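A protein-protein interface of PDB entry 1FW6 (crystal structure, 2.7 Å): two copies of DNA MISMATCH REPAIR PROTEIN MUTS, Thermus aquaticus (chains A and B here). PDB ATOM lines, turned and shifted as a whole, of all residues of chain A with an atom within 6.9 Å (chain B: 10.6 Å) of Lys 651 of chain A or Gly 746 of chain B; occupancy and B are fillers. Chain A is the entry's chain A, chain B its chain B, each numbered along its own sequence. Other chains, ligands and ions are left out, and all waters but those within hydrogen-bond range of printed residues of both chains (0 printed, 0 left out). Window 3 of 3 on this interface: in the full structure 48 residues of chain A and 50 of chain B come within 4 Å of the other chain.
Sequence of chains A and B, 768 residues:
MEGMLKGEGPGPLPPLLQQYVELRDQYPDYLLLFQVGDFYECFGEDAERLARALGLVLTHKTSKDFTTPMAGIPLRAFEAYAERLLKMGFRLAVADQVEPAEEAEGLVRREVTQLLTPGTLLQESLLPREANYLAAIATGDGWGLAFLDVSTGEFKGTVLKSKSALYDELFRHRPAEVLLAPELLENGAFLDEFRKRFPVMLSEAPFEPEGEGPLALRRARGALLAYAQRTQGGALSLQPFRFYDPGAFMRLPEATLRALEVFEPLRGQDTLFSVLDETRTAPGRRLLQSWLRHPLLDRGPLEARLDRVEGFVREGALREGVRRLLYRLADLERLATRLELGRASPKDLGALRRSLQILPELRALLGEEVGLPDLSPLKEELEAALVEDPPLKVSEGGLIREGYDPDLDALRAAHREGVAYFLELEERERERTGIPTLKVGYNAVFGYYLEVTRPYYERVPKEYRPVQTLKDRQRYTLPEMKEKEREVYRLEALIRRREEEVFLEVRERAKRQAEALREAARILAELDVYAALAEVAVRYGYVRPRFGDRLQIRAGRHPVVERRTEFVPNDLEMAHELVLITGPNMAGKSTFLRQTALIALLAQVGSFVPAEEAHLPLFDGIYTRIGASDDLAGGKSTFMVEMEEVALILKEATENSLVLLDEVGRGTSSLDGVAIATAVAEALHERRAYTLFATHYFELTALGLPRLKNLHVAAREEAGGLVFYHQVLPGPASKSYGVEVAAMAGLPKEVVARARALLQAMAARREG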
ATOM      1  N   MET A 640     -12.188 -30.057 -18.546  1.00  0.00           N
ATOM      2  CA  MET A 640     -11.904 -30.578 -17.223  1.00  0.00           C
ATOM      3  C   MET A 640     -11.031 -31.836 -17.283  1.00  0.00           C
ATOM      4  O   MET A 640     -10.064 -31.980 -16.525  1.00  0.00           O
ATOM      5  CB  MET A 640     -13.201 -30.867 -16.495  1.00  0.00           C
ATOM      6  CG  MET A 640     -12.984 -31.360 -15.099  1.00  0.00           C
ATOM      7  SD  MET A 640     -14.609 -31.284 -14.125  1.00  0.00           S
ATOM      8  CE  MET A 640     -13.850 -31.053 -12.360  1.00  0.00           C
ATOM      9  N   MET A 643      -7.590 -30.929 -18.039  1.00  0.00           N
ATOM     10  CA  MET A 643      -6.974 -30.276 -16.895  1.00  0.00           C
ATOM     11  C   MET A 643      -6.550 -31.303 -15.859  1.00  0.00           C
ATOM     12  O   MET A 643      -5.468 -31.194 -15.288  1.00  0.00           O
ATOM     13  CB  MET A 643      -7.928 -29.249 -16.274  1.00  0.00           C
ATOM     14  CG  MET A 643      -8.080 -27.971 -17.087  1.00  0.00           C
ATOM     15  SD  MET A 643      -6.372 -27.132 -17.456  1.00  0.00           S
ATOM     16  CE  MET A 643      -6.179 -27.515 -19.341  1.00  0.00           C
ATOM     17  N   GLU A 644      -7.385 -32.307 -15.616  1.00  0.00           N
ATOM     18  CA  GLU A 644      -7.013 -33.328 -14.651  1.00  0.00           C
ATOM     19  C   GLU A 644      -5.686 -33.975 -15.042  1.00  0.00           C
ATOM     20  O   GLU A 644      -4.876 -34.322 -14.184  1.00  0.00           O
ATOM     21  CB  GLU A 644      -8.082 -34.393 -14.570  1.00  0.00           C
ATOM     22  CG  GLU A 644      -9.402 -33.898 -14.066  1.00  0.00           C
ATOM     23  CD  GLU A 644     -10.423 -35.013 -14.020  1.00  0.00           C
ATOM     24  OE1 GLU A 644     -11.601 -34.744 -13.697  1.00  0.00           O
ATOM     25  OE2 GLU A 644     -10.039 -36.166 -14.311  1.00  0.00           O
ATOM     26  N   GLU A 645      -5.466 -34.148 -16.341  1.00  0.00           N
ATOM     27  CA  GLU A 645      -4.219 -34.731 -16.820  1.00  0.00           C
ATOM     28  C   GLU A 645      -3.044 -33.785 -16.559  1.00  0.00           C
ATOM     29  O   GLU A 645      -1.975 -34.206 -16.108  1.00  0.00           O
ATOM     30  CB  GLU A 645      -4.312 -35.025 -18.311  1.00  0.00           C
ATOM     31  CG  GLU A 645      -5.190 -36.203 -18.661  1.00  0.00           C
ATOM     32  CD  GLU A 645      -5.000 -36.650 -20.106  1.00  0.00           C
ATOM     33  OE1 GLU A 645      -3.837 -36.891 -20.505  1.00  0.00           O
ATOM     34  OE2 GLU A 645      -6.008 -36.766 -20.841  1.00  0.00           O
ATOM     35  N   VAL A 646      -3.234 -32.504 -16.845  1.00  0.00           N
ATOM     36  CA  VAL A 646      -2.167 -31.537 -16.616  1.00  0.00           C
ATOM     37  C   VAL A 646      -1.784 -31.585 -15.143  1.00  0.00           C
ATOM     38  O   VAL A 646      -0.615 -31.473 -14.795  1.00  0.00           O
ATOM     39  CB  VAL A 646      -2.609 -30.104 -16.988  1.00  0.00           C
ATOM     40  CG1 VAL A 646      -1.435 -29.157 -16.887  1.00  0.00           C
ATOM     41  CG2 VAL A 646      -3.178 -30.084 -18.396  1.00  0.00           C
ATOM     42  N   ALA A 647      -2.779 -31.761 -14.281  1.00  0.00           N
ATOM     43  CA  ALA A 647      -2.536 -31.851 -12.849  1.00  0.00           C
ATOM     44  C   ALA A 647      -1.578 -33.016 -12.604  1.00  0.00           C
ATOM     45  O   ALA A 647      -0.476 -32.831 -12.077  1.00  0.00           O
ATOM     46  CB  ALA A 647      -3.846 -32.078 -12.102  1.00  0.00           C
ATOM     47  N   LEU A 648      -1.992 -34.219 -12.988  1.00  0.00           N
ATOM     48  CA  LEU A 648      -1.137 -35.380 -12.805  1.00  0.00           C
ATOM     49  C   LEU A 648       0.256 -35.069 -13.331  1.00  0.00           C
ATOM     50  O   LEU A 648       1.222 -35.059 -12.575  1.00  0.00           O
ATOM     51  CB  LEU A 648      -1.698 -36.596 -13.547  1.00  0.00           C
ATOM     52  CG  LEU A 648      -2.925 -37.305 -12.975  1.00  0.00           C
ATOM     53  CD1 LEU A 648      -3.572 -38.176 -14.049  1.00  0.00           C
ATOM     54  CD2 LEU A 648      -2.513 -38.128 -11.775  1.00  0.00           C
ATOM     55  N   ILE A 649       0.358 -34.797 -14.628  1.00  0.00           N
ATOM     56  CA  ILE A 649       1.654 -34.505 -15.225  1.00  0.00           C
ATOM     57  C   ILE A 649       2.440 -33.512 -14.393  1.00  0.00           C
ATOM     58  O   ILE A 649       3.645 -33.644 -14.261  1.00  0.00           O
ATOM     59  CB  ILE A 649       1.522 -33.922 -16.638  1.00  0.00           C
ATOM     60  CG1 ILE A 649       0.904 -34.955 -17.576  1.00  0.00           C
ATOM     61  CG2 ILE A 649       2.894 -33.466 -17.136  1.00  0.00           C
ATOM     62  CD1 ILE A 649       0.600 -34.402 -18.943  1.00  0.00           C
ATOM     63  N   LEU A 650       1.758 -32.516 -13.834  1.00  0.00           N
ATOM     64  CA  LEU A 650       2.432 -31.506 -13.027  1.00  0.00           C
ATOM     65  C   LEU A 650       2.875 -32.003 -11.661  1.00  0.00           C
ATOM     66  O   LEU A 650       3.815 -31.463 -11.078  1.00  0.00           O
ATOM     67  CB  LEU A 650       1.546 -30.278 -12.845  1.00  0.00           C
ATOM     68  CG  LEU A 650       1.738 -29.159 -13.869  1.00  0.00           C
ATOM     69  CD1 LEU A 650       0.775 -28.018 -13.573  1.00  0.00           C
ATOM     70  CD2 LEU A 650       3.191 -28.681 -13.835  1.00  0.00           C
ATOM     71  N   LYS A 651       2.219 -33.037 -11.154  1.00  0.00           N
ATOM     72  CA  LYS A 651       2.567 -33.558  -9.842  1.00  0.00           C
ATOM     73  C   LYS A 651       3.633 -34.657  -9.836  1.00  0.00           C
ATOM     74  O   LYS A 651       4.003 -35.163  -8.777  1.00  0.00           O
ATOM     75  CB  LYS A 651       1.295 -34.033  -9.141  1.00  0.00           C
ATOM     76  CG  LYS A 651       0.294 -32.903  -8.951  1.00  0.00           C
ATOM     77  CD  LYS A 651      -1.006 -33.372  -8.311  1.00  0.00           C
ATOM     78  CE  LYS A 651      -2.009 -32.224  -8.204  1.00  0.00           C
ATOM     79  NZ  LYS A 651      -3.333 -32.695  -7.699  1.00  0.00           N
ATOM     80  N   GLU A 652       4.154 -35.011 -11.003  1.00  0.00           N
ATOM     81  CA  GLU A 652       5.163 -36.058 -11.048  1.00  0.00           C
ATOM     82  C   GLU A 652       6.331 -35.762 -11.961  1.00  0.00           C
ATOM     83  O   GLU A 652       7.369 -36.407 -11.871  1.00  0.00           O
ATOM     84  CB  GLU A 652       4.516 -37.374 -11.454  1.00  0.00           C
ATOM     85  CG  GLU A 652       3.538 -37.221 -12.581  1.00  0.00           C
ATOM     86  CD  GLU A 652       2.680 -38.446 -12.760  1.00  0.00           C
ATOM     87  OE1 GLU A 652       2.184 -38.958 -11.731  1.00  0.00           O
ATOM     88  OE2 GLU A 652       2.494 -38.887 -13.922  1.00  0.00           O
ATOM     89  N   ALA A 653       6.184 -34.787 -12.841  1.00  0.00           N
ATOM     90  CA  ALA A 653       7.283 -34.476 -13.730  1.00  0.00           C
ATOM     91  C   ALA A 653       8.440 -33.950 -12.897  1.00  0.00           C
ATOM     92  O   ALA A 653       8.235 -33.262 -11.904  1.00  0.00           O
ATOM     93  CB  ALA A 653       6.854 -33.436 -14.746  1.00  0.00           C
ATOM     94  N   ARG A 687       9.992 -26.187 -13.477  1.00  0.00           N
ATOM     95  CA  ARG A 687      10.279 -27.586 -13.172  1.00  0.00           C
ATOM     96  C   ARG A 687      11.590 -28.013 -13.850  1.00  0.00           C
ATOM     97  O   ARG A 687      12.365 -28.804 -13.301  1.00  0.00           O
ATOM     98  CB  ARG A 687       9.111 -28.469 -13.637  1.00  0.00           C
ATOM     99  CG  ARG A 687       9.145 -29.908 -13.126  1.00  0.00           C
ATOM    100  CD  ARG A 687       9.082 -29.990 -11.600  1.00  0.00           C
ATOM    101  NE  ARG A 687       7.881 -29.362 -11.048  1.00  0.00           N
ATOM    102  CZ  ARG A 687       6.642 -29.805 -11.242  1.00  0.00           C
ATOM    103  NH1 ARG A 687       6.427 -30.897 -11.974  1.00  0.00           N
ATOM    104  NH2 ARG A 687       5.613 -29.137 -10.726  1.00  0.00           N
ATOM    105  N   GLY B 721     -16.599 -26.362  -4.749  1.00  0.00           N
ATOM    106  CA  GLY B 721     -16.273 -25.558  -5.912  1.00  0.00           C
ATOM    107  C   GLY B 721     -17.457 -24.996  -6.678  1.00  0.00           C
ATOM    108  O   GLY B 721     -18.055 -23.995  -6.265  1.00  0.00           O
ATOM    109  N   GLY B 738     -13.102 -21.130 -16.715  1.00  0.00           N
ATOM    110  CA  GLY B 738     -11.946 -21.931 -17.070  1.00  0.00           C
ATOM    111  C   GLY B 738     -11.090 -22.192 -15.845  1.00  0.00           C
ATOM    112  O   GLY B 738     -11.042 -23.310 -15.325  1.00  0.00           O
ATOM    113  N   VAL B 739     -10.426 -21.139 -15.378  1.00  0.00           N
ATOM    114  CA  VAL B 739      -9.570 -21.224 -14.211  1.00  0.00           C
ATOM    115  C   VAL B 739     -10.299 -21.858 -13.025  1.00  0.00           C
ATOM    116  O   VAL B 739      -9.723 -22.662 -12.300  1.00  0.00           O
ATOM    117  CB  VAL B 739      -9.049 -19.829 -13.833  1.00  0.00           C
ATOM    118  CG1 VAL B 739      -8.062 -19.921 -12.683  1.00  0.00           C
ATOM    119  CG2 VAL B 739      -8.368 -19.204 -15.039  1.00  0.00           C
ATOM    120  N   GLU B 740     -11.566 -21.510 -12.830  1.00  0.00           N
ATOM    121  CA  GLU B 740     -12.333 -22.090 -11.730  1.00  0.00           C
ATOM    122  C   GLU B 740     -12.408 -23.602 -11.880  1.00  0.00           C
ATOM    123  O   GLU B 740     -12.410 -24.338 -10.894  1.00  0.00           O
ATOM    124  CB  GLU B 740     -13.757 -21.528 -11.689  1.00  0.00           C
ATOM    125  CG  GLU B 740     -13.934 -20.309 -10.798  1.00  0.00           C
ATOM    126  CD  GLU B 740     -13.067 -19.143 -11.241  1.00  0.00           C
ATOM    127  OE1 GLU B 740     -13.246 -18.673 -12.395  1.00  0.00           O
ATOM    128  OE2 GLU B 740     -12.206 -18.701 -10.438  1.00  0.00           O
ATOM    129  N   VAL B 741     -12.463 -24.063 -13.123  1.00  0.00           N
ATOM    130  CA  VAL B 741     -12.566 -25.488 -13.397  1.00  0.00           C
ATOM    131  C   VAL B 741     -11.226 -26.206 -13.303  1.00  0.00           C
ATOM    132  O   VAL B 741     -11.168 -27.357 -12.866  1.00  0.00           O
ATOM    133  CB  VAL B 741     -13.212 -25.717 -14.776  1.00  0.00           C
ATOM    134  CG1 VAL B 741     -13.310 -27.198 -15.083  1.00  0.00           C
ATOM    135  CG2 VAL B 741     -14.583 -25.082 -14.782  1.00  0.00           C
ATOM    136  N   ALA B 742     -10.151 -25.538 -13.702  1.00  0.00           N
ATOM    137  CA  ALA B 742      -8.840 -26.156 -13.618  1.00  0.00           C
ATOM    138  C   ALA B 742      -8.573 -26.382 -12.138  1.00  0.00           C
ATOM    139  O   ALA B 742      -7.879 -27.329 -11.749  1.00  0.00           O
ATOM    140  CB  ALA B 742      -7.776 -25.244 -14.218  1.00  0.00           C
ATOM    141  N   ALA B 743      -9.143 -25.499 -11.321  1.00  0.00           N
ATOM    142  CA  ALA B 743      -8.986 -25.560  -9.869  1.00  0.00           C
ATOM    143  C   ALA B 743      -9.589 -26.864  -9.339  1.00  0.00           C
ATOM    144  O   ALA B 743      -8.938 -27.623  -8.623  1.00  0.00           O
ATOM    145  CB  ALA B 743      -9.658 -24.354  -9.227  1.00  0.00           C
ATOM    146  N   MET B 744     -10.841 -27.117  -9.686  1.00  0.00           N
ATOM    147  CA  MET B 744     -11.481 -28.342  -9.268  1.00  0.00           C
ATOM    148  C   MET B 744     -10.725 -29.514  -9.891  1.00  0.00           C
ATOM    149  O   MET B 744     -10.608 -30.589  -9.293  1.00  0.00           O
ATOM    150  CB  MET B 744     -12.908 -28.382  -9.766  1.00  0.00           C
ATOM    151  CG  MET B 744     -13.786 -27.273  -9.304  1.00  0.00           C
ATOM    152  SD  MET B 744     -15.521 -27.736  -9.989  1.00  0.00           S
ATOM    153  CE  MET B 744     -15.744 -26.272 -11.232  1.00  0.00           C
ATOM    154  N   ALA B 745     -10.225 -29.307 -11.106  1.00  0.00           N
ATOM    155  CA  ALA B 745      -9.485 -30.349 -11.816  1.00  0.00           C
ATOM    156  C   ALA B 745      -8.316 -30.859 -10.995  1.00  0.00           C
ATOM    157  O   ALA B 745      -7.936 -32.017 -11.112  1.00  0.00           O
ATOM    158  CB  ALA B 745      -8.978 -29.820 -13.150  1.00  0.00           C
ATOM    159  N   GLY B 746      -7.736 -29.983 -10.178  1.00  0.00           N
ATOM    160  CA  GLY B 746      -6.620 -30.386  -9.352  1.00  0.00           C
ATOM    161  C   GLY B 746      -5.337 -29.661  -9.665  1.00  0.00           C
ATOM    162  O   GLY B 746      -4.278 -30.043  -9.177  1.00  0.00           O
ATOM    163  N   LEU B 747      -5.425 -28.616 -10.482  1.00  0.00           N
ATOM    164  CA  LEU B 747      -4.251 -27.827 -10.852  1.00  0.00           C
ATOM    165  C   LEU B 747      -3.620 -27.143  -9.619  1.00  0.00           C
ATOM    166  O   LEU B 747      -4.308 -26.492  -8.817  1.00  0.00           O
ATOM    167  CB  LEU B 747      -4.644 -26.748 -11.872  1.00  0.00           C
ATOM    168  CG  LEU B 747      -3.874 -26.572 -13.184  1.00  0.00           C
ATOM    169  CD1 LEU B 747      -2.399 -26.813 -12.972  1.00  0.00           C
ATOM    170  CD2 LEU B 747      -4.394 -27.548 -14.203  1.00  0.00           C
ATOM    171  N   PRO B 748      -2.299 -27.279  -9.457  1.00  0.00           N
ATOM    172  CA  PRO B 748      -1.575 -26.678  -8.336  1.00  0.00           C
ATOM    173  C   PRO B 748      -1.985 -25.227  -8.093  1.00  0.00           C
ATOM    174  O   PRO B 748      -1.923 -24.391  -9.002  1.00  0.00           O
ATOM    175  CB  PRO B 748      -0.128 -26.787  -8.777  1.00  0.00           C
ATOM    176  CG  PRO B 748      -0.122 -28.079  -9.506  1.00  0.00           C
ATOM    177  CD  PRO B 748      -1.375 -28.005 -10.341  1.00  0.00           C
ATOM    178  N   LYS B 749      -2.388 -24.943  -6.856  1.00  0.00           N
ATOM    179  CA  LYS B 749      -2.827 -23.612  -6.447  1.00  0.00           C
ATOM    180  C   LYS B 749      -1.993 -22.471  -7.000  1.00  0.00           C
ATOM    181  O   LYS B 749      -2.536 -21.421  -7.341  1.00  0.00           O
ATOM    182  CB  LYS B 749      -2.864 -23.531  -4.922  1.00  0.00           C
ATOM    183  CG  LYS B 749      -3.855 -24.516  -4.332  1.00  0.00           C
ATOM    184  CD  LYS B 749      -3.649 -24.766  -2.854  1.00  0.00           C
ATOM    185  CE  LYS B 749      -4.576 -25.887  -2.380  1.00  0.00           C
ATOM    186  NZ  LYS B 749      -4.375 -26.220  -0.933  1.00  0.00           N
ATOM    187  N   GLU B 750      -0.681 -22.666  -7.101  1.00  0.00           N
ATOM    188  CA  GLU B 750       0.175 -21.601  -7.611  1.00  0.00           C
ATOM    189  C   GLU B 750      -0.155 -21.344  -9.071  1.00  0.00           C
ATOM    190  O   GLU B 750      -0.334 -20.191  -9.484  1.00  0.00           O
ATOM    191  CB  GLU B 750       1.660 -21.961  -7.485  1.00  0.00           C
ATOM    192  CG  GLU B 750       2.032 -22.615  -6.177  1.00  0.00           C
ATOM    193  CD  GLU B 750       1.801 -24.115  -6.212  1.00  0.00           C
ATOM    194  OE1 GLU B 750       2.582 -24.805  -6.910  1.00  0.00           O
ATOM    195  OE2 GLU B 750       0.842 -24.602  -5.560  1.00  0.00           O
ATOM    196  N   VAL B 751      -0.239 -22.423  -9.851  1.00  0.00           N
ATOM    197  CA  VAL B 751      -0.539 -22.304 -11.272  1.00  0.00           C
ATOM    198  C   VAL B 751      -1.902 -21.657 -11.427  1.00  0.00           C
ATOM    199  O   VAL B 751      -2.098 -20.803 -12.291  1.00  0.00           O
ATOM    200  CB  VAL B 751      -0.563 -23.666 -11.967  1.00  0.00           C
ATOM    201  CG1 VAL B 751      -0.638 -23.471 -13.467  1.00  0.00           C
ATOM    202  CG2 VAL B 751       0.660 -24.466 -11.580  1.00  0.00           C
ATOM    203  N   VAL B 752      -2.852 -22.064 -10.594  1.00  0.00           N
ATOM    204  CA  VAL B 752      -4.181 -21.474 -10.651  1.00  0.00           C
ATOM    205  C   VAL B 752      -4.098 -19.968 -10.354  1.00  0.00           C
ATOM    206  O   VAL B 752      -4.654 -19.142 -11.091  1.00  0.00           O
ATOM    207  CB  VAL B 752      -5.120 -22.136  -9.633  1.00  0.00           C
ATOM    208  CG1 VAL B 752      -6.470 -21.458  -9.650  1.00  0.00           C
ATOM    209  CG2 VAL B 752      -5.253 -23.604  -9.949  1.00  0.00           C
ATOM    210  N   ALA B 753      -3.393 -19.627  -9.277  1.00  0.00           N
ATOM    211  CA  ALA B 753      -3.228 -18.241  -8.856  1.00  0.00           C
ATOM    212  C   ALA B 753      -2.562 -17.421  -9.954  1.00  0.00           C
ATOM    213  O   ALA B 753      -2.969 -16.288 -10.242  1.00  0.00           O
ATOM    214  CB  ALA B 753      -2.407 -18.184  -7.593  1.00  0.00           C
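The side-chain amino group (NZ) of Lys 651 of chain A is in hydrogen-bond range of the backbone carbonyl oxygen (O) of Gly 746 of chain B, at 3.2 Å.
The guanidinium group (NH1) of Arg 687 of chain A sits at hydrogen-bond distance from the backbone carbonyl oxygen (O) of Leu 650 of chain A (2.8 Å).
The backbone carbonyl oxygen (O) of Ala 742 of chain B is in hydrogen-bond range of the backbone NH (N) of Leu 747 of chain B (3.0 Å).
Among the printed residues, merely in contact across the chains: Met 643 of chain A with Ala 745 of chain B (3.3 Å), Leu 650 of chain A with Leu 747 of chain B (3.4 Å), Ala 647 of chain A with Gly 746 of chain B (3.6 Å), Glu 644 of chain A with Ala 745 of chain B (3.8 Å), Met 643 of chain A with Leu 747 of chain B (3.8 Å), Met 640 of chain A with Met 744 of chain B (3.8 Å), Leu 650 of chain A with Pro 748 of chain B (3.9 Å), Met 640 of chain A with Val 741 of chain B (3.9 Å) and Met 643 of chain A with Ala 742 of chain B (3.97 Å).
Printed residues of chain B within 4 Å of Glu 644 of chain A: Ala 745 (3.8 Å).
Of chain B, only Gly 746 (3.6 Å) comes within 4 Å of Ala 647 of chain A.
Leu 650 of chain A touches two residues of chain B.
Of the printed residues of chain B, Lys 651 of chain A touches Gly 746.
No residue of chain B comes within 4 Å of Glu 652 of chain A.
Ala 653 of chain A touches none of the printed residues of chain B.
Printed residues of chain A within 4 Å of Val 741 of chain B: Met 640.
Printed residues of chain A within 4 Å of Met 744 of chain B: Met 640 (3.8 Å).
Gly 746 of chain B touches just these residues of chain A: Ala 647 and Lys 651.
Printed residues of chain A within 4 Å of Leu 747 of chain B: Met 643 (3.8 Å) and Leu 650 (3.4 Å).
Of the printed residues of chain A, Pro 748 of chain B touches Leu 650 (3.9 Å).
The nearest residue of chain B that does not touch Lys 651 of chain A is Pro 748 of chain B (4.7 Å).
The nearest printed residue of chain B that does not touch Glu 644 of chain A is Gly 746 of chain B (5.6 Å).
Hydrophobic or aromatic side chains of chain A that line the printed part of chain B: Met 640, Met 643, Ala 647 and Leu 650.
Of the 17 printed residues of chain B, 7 touch a printed residue of chain A.
Printed residues of chain B that touch a printed residue of chain A: Val 741, Ala 742, Met 744, Ala 745, Gly 746, Leu 747 and Pro 748.
Along chain B the printed residues that touch a printed residue of chain A span positions 741 to 748.
Among the printed residues, 10 pairs touch across the chains.
No position is printed for both chains.
Of the 10 pairs that touch across the chains among the printed residues, none has its exchanged pair printed and touching as well.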
